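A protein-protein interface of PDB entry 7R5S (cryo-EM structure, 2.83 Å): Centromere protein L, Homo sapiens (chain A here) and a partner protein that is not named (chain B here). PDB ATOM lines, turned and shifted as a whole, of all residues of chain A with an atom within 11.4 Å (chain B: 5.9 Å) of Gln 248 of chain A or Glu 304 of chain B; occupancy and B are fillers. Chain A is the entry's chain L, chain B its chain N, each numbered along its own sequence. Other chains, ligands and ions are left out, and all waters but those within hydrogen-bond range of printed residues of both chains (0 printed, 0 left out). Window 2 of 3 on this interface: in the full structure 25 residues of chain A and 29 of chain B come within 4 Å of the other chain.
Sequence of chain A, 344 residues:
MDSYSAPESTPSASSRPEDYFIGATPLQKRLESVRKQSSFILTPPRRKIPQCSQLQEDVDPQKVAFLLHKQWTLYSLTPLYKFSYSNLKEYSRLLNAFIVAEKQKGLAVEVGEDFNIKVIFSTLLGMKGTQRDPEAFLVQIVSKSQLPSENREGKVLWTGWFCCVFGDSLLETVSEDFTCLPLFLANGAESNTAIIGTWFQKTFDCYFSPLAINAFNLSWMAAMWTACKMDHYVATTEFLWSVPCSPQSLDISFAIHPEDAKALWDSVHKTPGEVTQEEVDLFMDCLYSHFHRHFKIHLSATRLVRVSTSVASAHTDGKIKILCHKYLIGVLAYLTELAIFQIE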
ATOM      1  N   TRP A 241      27.154  23.416  11.617  1.00  0.00           N
ATOM      2  CA  TRP A 241      27.467  22.036  11.959  1.00  0.00           C
ATOM      3  C   TRP A 241      26.986  21.105  10.856  1.00  0.00           C
ATOM      4  O   TRP A 241      25.910  21.307  10.282  1.00  0.00           O
ATOM      5  CB  TRP A 241      26.822  21.633  13.289  1.00  0.00           C
ATOM      6  CG  TRP A 241      27.617  22.022  14.495  1.00  0.00           C
ATOM      7  CD1 TRP A 241      28.742  21.411  14.968  1.00  0.00           C
ATOM      8  CD2 TRP A 241      27.342  23.104  15.392  1.00  0.00           C
ATOM      9  NE1 TRP A 241      29.188  22.048  16.099  1.00  0.00           N
ATOM     10  CE2 TRP A 241      28.345  23.091  16.381  1.00  0.00           C
ATOM     11  CE3 TRP A 241      26.347  24.083  15.454  1.00  0.00           C
ATOM     12  CZ2 TRP A 241      28.382  24.019  17.419  1.00  0.00           C
ATOM     13  CZ3 TRP A 241      26.384  25.002  16.485  1.00  0.00           C
ATOM     14  CH2 TRP A 241      27.395  24.964  17.452  1.00  0.00           C
ATOM     15  N   SER A 242      27.786  20.081  10.571  1.00  0.00           N
ATOM     16  CA  SER A 242      27.454  19.057   9.587  1.00  0.00           C
ATOM     17  C   SER A 242      27.210  17.744  10.316  1.00  0.00           C
ATOM     18  O   SER A 242      28.133  17.177  10.908  1.00  0.00           O
ATOM     19  CB  SER A 242      28.575  18.904   8.558  1.00  0.00           C
ATOM     20  OG  SER A 242      28.175  18.061   7.493  1.00  0.00           O
ATOM     21  N   VAL A 243      25.971  17.265  10.270  1.00  0.00           N
ATOM     22  CA  VAL A 243      25.582  16.041  10.968  1.00  0.00           C
ATOM     23  C   VAL A 243      25.998  14.835  10.136  1.00  0.00           C
ATOM     24  O   VAL A 243      25.595  14.722   8.970  1.00  0.00           O
ATOM     25  CB  VAL A 243      24.071  16.019  11.249  1.00  0.00           C
ATOM     26  CG1 VAL A 243      23.696  14.769  12.026  1.00  0.00           C
ATOM     27  CG2 VAL A 243      23.655  17.270  12.005  1.00  0.00           C
ATOM     28  N   PRO A 244      26.797  13.913  10.681  1.00  0.00           N
ATOM     29  CA  PRO A 244      27.176  12.728   9.901  1.00  0.00           C
ATOM     30  C   PRO A 244      26.035  11.731   9.787  1.00  0.00           C
ATOM     31  O   PRO A 244      25.742  10.983  10.725  1.00  0.00           O
ATOM     32  CB  PRO A 244      28.357  12.153  10.691  1.00  0.00           C
ATOM     33  CG  PRO A 244      28.122  12.606  12.091  1.00  0.00           C
ATOM     34  CD  PRO A 244      27.454  13.950  11.999  1.00  0.00           C
ATOM     35  N   CYS A 245      25.388  11.720   8.626  1.00  0.00           N
ATOM     36  CA  CYS A 245      24.282  10.815   8.327  1.00  0.00           C
ATOM     37  C   CYS A 245      24.427  10.308   6.897  1.00  0.00           C
ATOM     38  O   CYS A 245      23.474  10.304   6.119  1.00  0.00           O
ATOM     39  CB  CYS A 245      22.934  11.499   8.543  1.00  0.00           C
ATOM     40  SG  CYS A 245      22.808  13.154   7.831  1.00  0.00           S
ATOM     41  N   SER A 246      25.643   9.864   6.552  1.00  0.00           N
ATOM     42  CA  SER A 246      26.165   9.642   5.202  1.00  0.00           C
ATOM     43  C   SER A 246      25.135   9.167   4.175  1.00  0.00           C
ATOM     44  O   SER A 246      25.147   9.666   3.042  1.00  0.00           O
ATOM     45  CB  SER A 246      27.334   8.654   5.255  1.00  0.00           C
ATOM     46  OG  SER A 246      28.223   8.975   6.312  1.00  0.00           O
ATOM     47  N   PRO A 247      24.248   8.211   4.491  1.00  0.00           N
ATOM     48  CA  PRO A 247      23.143   7.936   3.554  1.00  0.00           C
ATOM     49  C   PRO A 247      22.311   9.167   3.227  1.00  0.00           C
ATOM     50  O   PRO A 247      21.963   9.385   2.060  1.00  0.00           O
ATOM     51  CB  PRO A 247      22.323   6.870   4.291  1.00  0.00           C
ATOM     52  CG  PRO A 247      23.313   6.167   5.134  1.00  0.00           C
ATOM     53  CD  PRO A 247      24.276   7.226   5.591  1.00  0.00           C
ATOM     54  N   GLN A 248      21.983   9.976   4.228  1.00  0.00           N
ATOM     55  CA  GLN A 248      21.253  11.219   4.049  1.00  0.00           C
ATOM     56  C   GLN A 248      22.219  12.400   4.150  1.00  0.00           C
ATOM     57  O   GLN A 248      23.442  12.235   4.172  1.00  0.00           O
ATOM     58  CB  GLN A 248      20.124  11.312   5.076  1.00  0.00           C
ATOM     59  CG  GLN A 248      19.305  10.038   5.219  1.00  0.00           C
ATOM     60  CD  GLN A 248      18.471   9.734   3.990  1.00  0.00           C
ATOM     61  OE1 GLN A 248      18.194  10.617   3.178  1.00  0.00           O
ATOM     62  NE2 GLN A 248      18.065   8.479   3.847  1.00  0.00           N
ATOM     63  N   SER A 249      21.669  13.613   4.193  1.00  0.00           N
ATOM     64  CA  SER A 249      22.462  14.820   4.369  1.00  0.00           C
ATOM     65  C   SER A 249      21.676  15.814   5.211  1.00  0.00           C
ATOM     66  O   SER A 249      20.448  15.892   5.116  1.00  0.00           O
ATOM     67  CB  SER A 249      22.842  15.449   3.022  1.00  0.00           C
ATOM     68  OG  SER A 249      23.725  16.542   3.201  1.00  0.00           O
ATOM     69  N   LEU A 250      22.395  16.573   6.037  1.00  0.00           N
ATOM     70  CA  LEU A 250      21.759  17.528   6.936  1.00  0.00           C
ATOM     71  C   LEU A 250      22.805  18.495   7.468  1.00  0.00           C
ATOM     72  O   LEU A 250      23.905  18.081   7.841  1.00  0.00           O
ATOM     73  CB  LEU A 250      21.060  16.813   8.100  1.00  0.00           C
ATOM     74  CG  LEU A 250      20.322  17.697   9.106  1.00  0.00           C
ATOM     75  CD1 LEU A 250      19.197  18.457   8.427  1.00  0.00           C
ATOM     76  CD2 LEU A 250      19.787  16.864  10.260  1.00  0.00           C
ATOM     77  N   ASP A 251      22.454  19.780   7.495  1.00  0.00           N
ATOM     78  CA  ASP A 251      23.292  20.823   8.068  1.00  0.00           C
ATOM     79  C   ASP A 251      22.466  21.647   9.044  1.00  0.00           C
ATOM     80  O   ASP A 251      21.261  21.833   8.855  1.00  0.00           O
ATOM     81  CB  ASP A 251      23.884  21.735   6.986  1.00  0.00           C
ATOM     82  CG  ASP A 251      24.882  21.017   6.100  1.00  0.00           C
ATOM     83  OD1 ASP A 251      24.466  20.117   5.341  1.00  0.00           O
ATOM     84  OD2 ASP A 251      26.083  21.354   6.162  1.00  0.00           O
ATOM     85  N   PRO B 260       5.556   7.145   2.941  1.00  0.00           N
ATOM     86  CA  PRO B 260       6.652   7.935   2.366  1.00  0.00           C
ATOM     87  C   PRO B 260       6.557   9.393   2.796  1.00  0.00           C
ATOM     88  O   PRO B 260       5.511  10.031   2.668  1.00  0.00           O
ATOM     89  CB  PRO B 260       6.451   7.774   0.855  1.00  0.00           C
ATOM     90  CG  PRO B 260       5.667   6.513   0.708  1.00  0.00           C
ATOM     91  CD  PRO B 260       4.767   6.460   1.904  1.00  0.00           C
ATOM     92  N   GLN B 261       7.665   9.914   3.310  1.00  0.00           N
ATOM     93  CA  GLN B 261       7.671  11.272   3.831  1.00  0.00           C
ATOM     94  C   GLN B 261       7.656  12.280   2.683  1.00  0.00           C
ATOM     95  O   GLN B 261       8.327  12.076   1.668  1.00  0.00           O
ATOM     96  CB  GLN B 261       8.900  11.503   4.709  1.00  0.00           C
ATOM     97  CG  GLN B 261       9.087  10.471   5.809  1.00  0.00           C
ATOM     98  CD  GLN B 261       8.025  10.566   6.886  1.00  0.00           C
ATOM     99  OE1 GLN B 261       7.454  11.630   7.119  1.00  0.00           O
ATOM    100  NE2 GLN B 261       7.756   9.448   7.551  1.00  0.00           N
ATOM    101  N   HIS B 301      16.737  16.404   1.337  1.00  0.00           N
ATOM    102  CA  HIS B 301      15.467  15.714   1.581  1.00  0.00           C
ATOM    103  C   HIS B 301      15.234  15.722   3.091  1.00  0.00           C
ATOM    104  O   HIS B 301      15.645  14.798   3.798  1.00  0.00           O
ATOM    105  CB  HIS B 301      15.486  14.300   1.015  1.00  0.00           C
ATOM    106  CG  HIS B 301      14.147  13.629   1.004  1.00  0.00           C
ATOM    107  ND1 HIS B 301      13.073  14.090   1.736  1.00  0.00           N
ATOM    108  CD2 HIS B 301      13.708  12.529   0.347  1.00  0.00           C
ATOM    109  CE1 HIS B 301      12.033  13.303   1.531  1.00  0.00           C
ATOM    110  NE2 HIS B 301      12.391  12.349   0.692  1.00  0.00           N
ATOM    111  N   LEU B 302      14.574  16.769   3.576  1.00  0.00           N
ATOM    112  CA  LEU B 302      14.223  16.838   4.984  1.00  0.00           C
ATOM    113  C   LEU B 302      13.121  15.827   5.296  1.00  0.00           C
ATOM    114  O   LEU B 302      12.487  15.261   4.401  1.00  0.00           O
ATOM    115  CB  LEU B 302      13.786  18.254   5.358  1.00  0.00           C
ATOM    116  CG  LEU B 302      13.972  18.677   6.818  1.00  0.00           C
ATOM    117  CD1 LEU B 302      15.435  18.594   7.218  1.00  0.00           C
ATOM    118  CD2 LEU B 302      13.430  20.077   7.046  1.00  0.00           C
ATOM    119  N   LEU B 303      12.910  15.591   6.592  1.00  0.00           N
ATOM    120  CA  LEU B 303      11.984  14.607   7.147  1.00  0.00           C
ATOM    121  C   LEU B 303      12.426  13.176   6.871  1.00  0.00           C
ATOM    122  O   LEU B 303      11.771  12.238   7.340  1.00  0.00           O
ATOM    123  CB  LEU B 303      10.545  14.793   6.643  1.00  0.00           C
ATOM    124  CG  LEU B 303       9.854  16.104   7.017  1.00  0.00           C
ATOM    125  CD1 LEU B 303       8.474  16.180   6.385  1.00  0.00           C
ATOM    126  CD2 LEU B 303       9.762  16.249   8.526  1.00  0.00           C
ATOM    127  N   GLU B 304      13.514  12.976   6.130  1.00  0.00           N
ATOM    128  CA  GLU B 304      14.111  11.663   5.933  1.00  0.00           C
ATOM    129  C   GLU B 304      15.455  11.516   6.621  1.00  0.00           C
ATOM    130  O   GLU B 304      15.802  10.412   7.044  1.00  0.00           O
ATOM    131  CB  GLU B 304      14.281  11.373   4.437  1.00  0.00           C
ATOM    132  CG  GLU B 304      14.440   9.901   4.100  1.00  0.00           C
ATOM    133  CD  GLU B 304      13.136   9.134   4.198  1.00  0.00           C
ATOM    134  OE1 GLU B 304      12.065   9.775   4.206  1.00  0.00           O
ATOM    135  OE2 GLU B 304      13.182   7.888   4.269  1.00  0.00           O
ATOM    136  N   ALA B 305      16.217  12.605   6.742  1.00  0.00           N
ATOM    137  CA  ALA B 305      17.452  12.578   7.514  1.00  0.00           C
ATOM    138  C   ALA B 305      17.182  12.595   9.012  1.00  0.00           C
ATOM    139  O   ALA B 305      17.946  12.002   9.781  1.00  0.00           O
ATOM    140  CB  ALA B 305      18.341  13.761   7.128  1.00  0.00           C
ATOM    141  N   LEU B 306      16.112  13.268   9.442  1.00  0.00           N
ATOM    142  CA  LEU B 306      15.764  13.278  10.858  1.00  0.00           C
ATOM    143  C   LEU B 306      15.314  11.900  11.324  1.00  0.00           C
ATOM    144  O   LEU B 306      15.669  11.463  12.426  1.00  0.00           O
ATOM    145  CB  LEU B 306      14.671  14.315  11.122  1.00  0.00           C
ATOM    146  CG  LEU B 306      14.968  15.757  10.710  1.00  0.00           C
ATOM    147  CD1 LEU B 306      13.742  16.632  10.909  1.00  0.00           C
ATOM    148  CD2 LEU B 306      16.151  16.308  11.489  1.00  0.00           C
ATOM    149  N   LYS B 307      14.538  11.198  10.492  1.00  0.00           N
ATOM    150  CA  LYS B 307      14.044   9.875  10.858  1.00  0.00           C
ATOM    151  C   LYS B 307      15.183   8.904  11.142  1.00  0.00           C
ATOM    152  O   LYS B 307      15.016   7.965  11.930  1.00  0.00           O
ATOM    153  CB  LYS B 307      13.144   9.334   9.746  1.00  0.00           C
ATOM    154  CG  LYS B 307      12.477   8.006  10.058  1.00  0.00           C
ATOM    155  CD  LYS B 307      11.680   7.501   8.867  1.00  0.00           C
ATOM    156  CE  LYS B 307      11.030   6.162   9.166  1.00  0.00           C
ATOM    157  NZ  LYS B 307      10.266   5.645   7.998  1.00  0.00           N
ATOM    158  N   SER B 308      16.342   9.115  10.526  1.00  0.00           N
ATOM    159  CA  SER B 308      17.499   8.255  10.723  1.00  0.00           C
ATOM    160  C   SER B 308      18.456   8.780  11.787  1.00  0.00           C
ATOM    161  O   SER B 308      19.582   8.283  11.886  1.00  0.00           O
ATOM    162  CB  SER B 308      18.248   8.072   9.401  1.00  0.00           C
ATOM    163  OG  SER B 308      18.638   9.323   8.860  1.00  0.00           O
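The backbone carbonyl oxygen (O) of Leu 250 of chain A is in hydrogen-bond range of the backbone NH (N) of Val 243 of chain A (3.3 Å). OG of Ser 308 of chain B sits at hydrogen-bond distance from O of Ala 305 of chain B (2.9 Å).
Among the printed residues, merely in contact across the chains: Ser 249 of chain A with Ala 305 of chain B, Gln 248 of chain A with Ala 305 of chain B, Gln 248 of chain A with Ser 308 of chain B, Leu 250 of chain A with Leu 306 of chain B, Gln 248 of chain A with Glu 304 of chain B and Leu 250 of chain A with Leu 302 of chain B.
Gln 248 of chain A touches just these residues of chain B: Glu 304 (3.9 Å), Ala 305 (3.7 Å) and Ser 308 (3.8 Å). Printed residues of chain B within 4 Å of Ser 249 of chain A: Ala 305 (3.6 Å). Of the printed residues of chain B, Leu 250 of chain A touches Leu 302 (3.95 Å) and Leu 306 (3.9 Å). His 301 of chain B touches none of the printed residues of chain A. Of the printed residues of chain A, Leu 302 of chain B touches Leu 250. No residue of chain A comes within 4 Å of Leu 303 of chain B. Of chain A, only Gln 248 and Ser 249 come within 4 Å of Ala 305 of chain B. Of chain A, only Leu 250 comes within 4 Å of Leu 306 of chain B. Ser 308 of chain B touches one residue of chain A. The nearest residue of chain A that does not touch Glu 304 of chain B is Ser 249 of chain A (6.8 Å). The nearest printed residue of chain B that does not touch Ser 249 of chain A is His 301 of chain B (5.1 Å).
Of the 11 printed residues of chain A, 3 touch a printed residue of chain B. Printed residues of chain A that touch a printed residue of chain B: Gln 248, Ser 249 and Leu 250. Of the 10 printed residues of chain B, 5 touch a printed residue of chain A. Printed residues of chain B that touch a printed residue of chain A: Leu 302, Glu 304, Ala 305, Leu 306 and Ser 308. Along chain B the printed residues that touch a printed residue of chain A span positions 302 to 308. Among the printed residues, no Asp or Glu carboxylate lies within 4 Å of a Lys or Arg side-chain nitrogen of the other chain.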
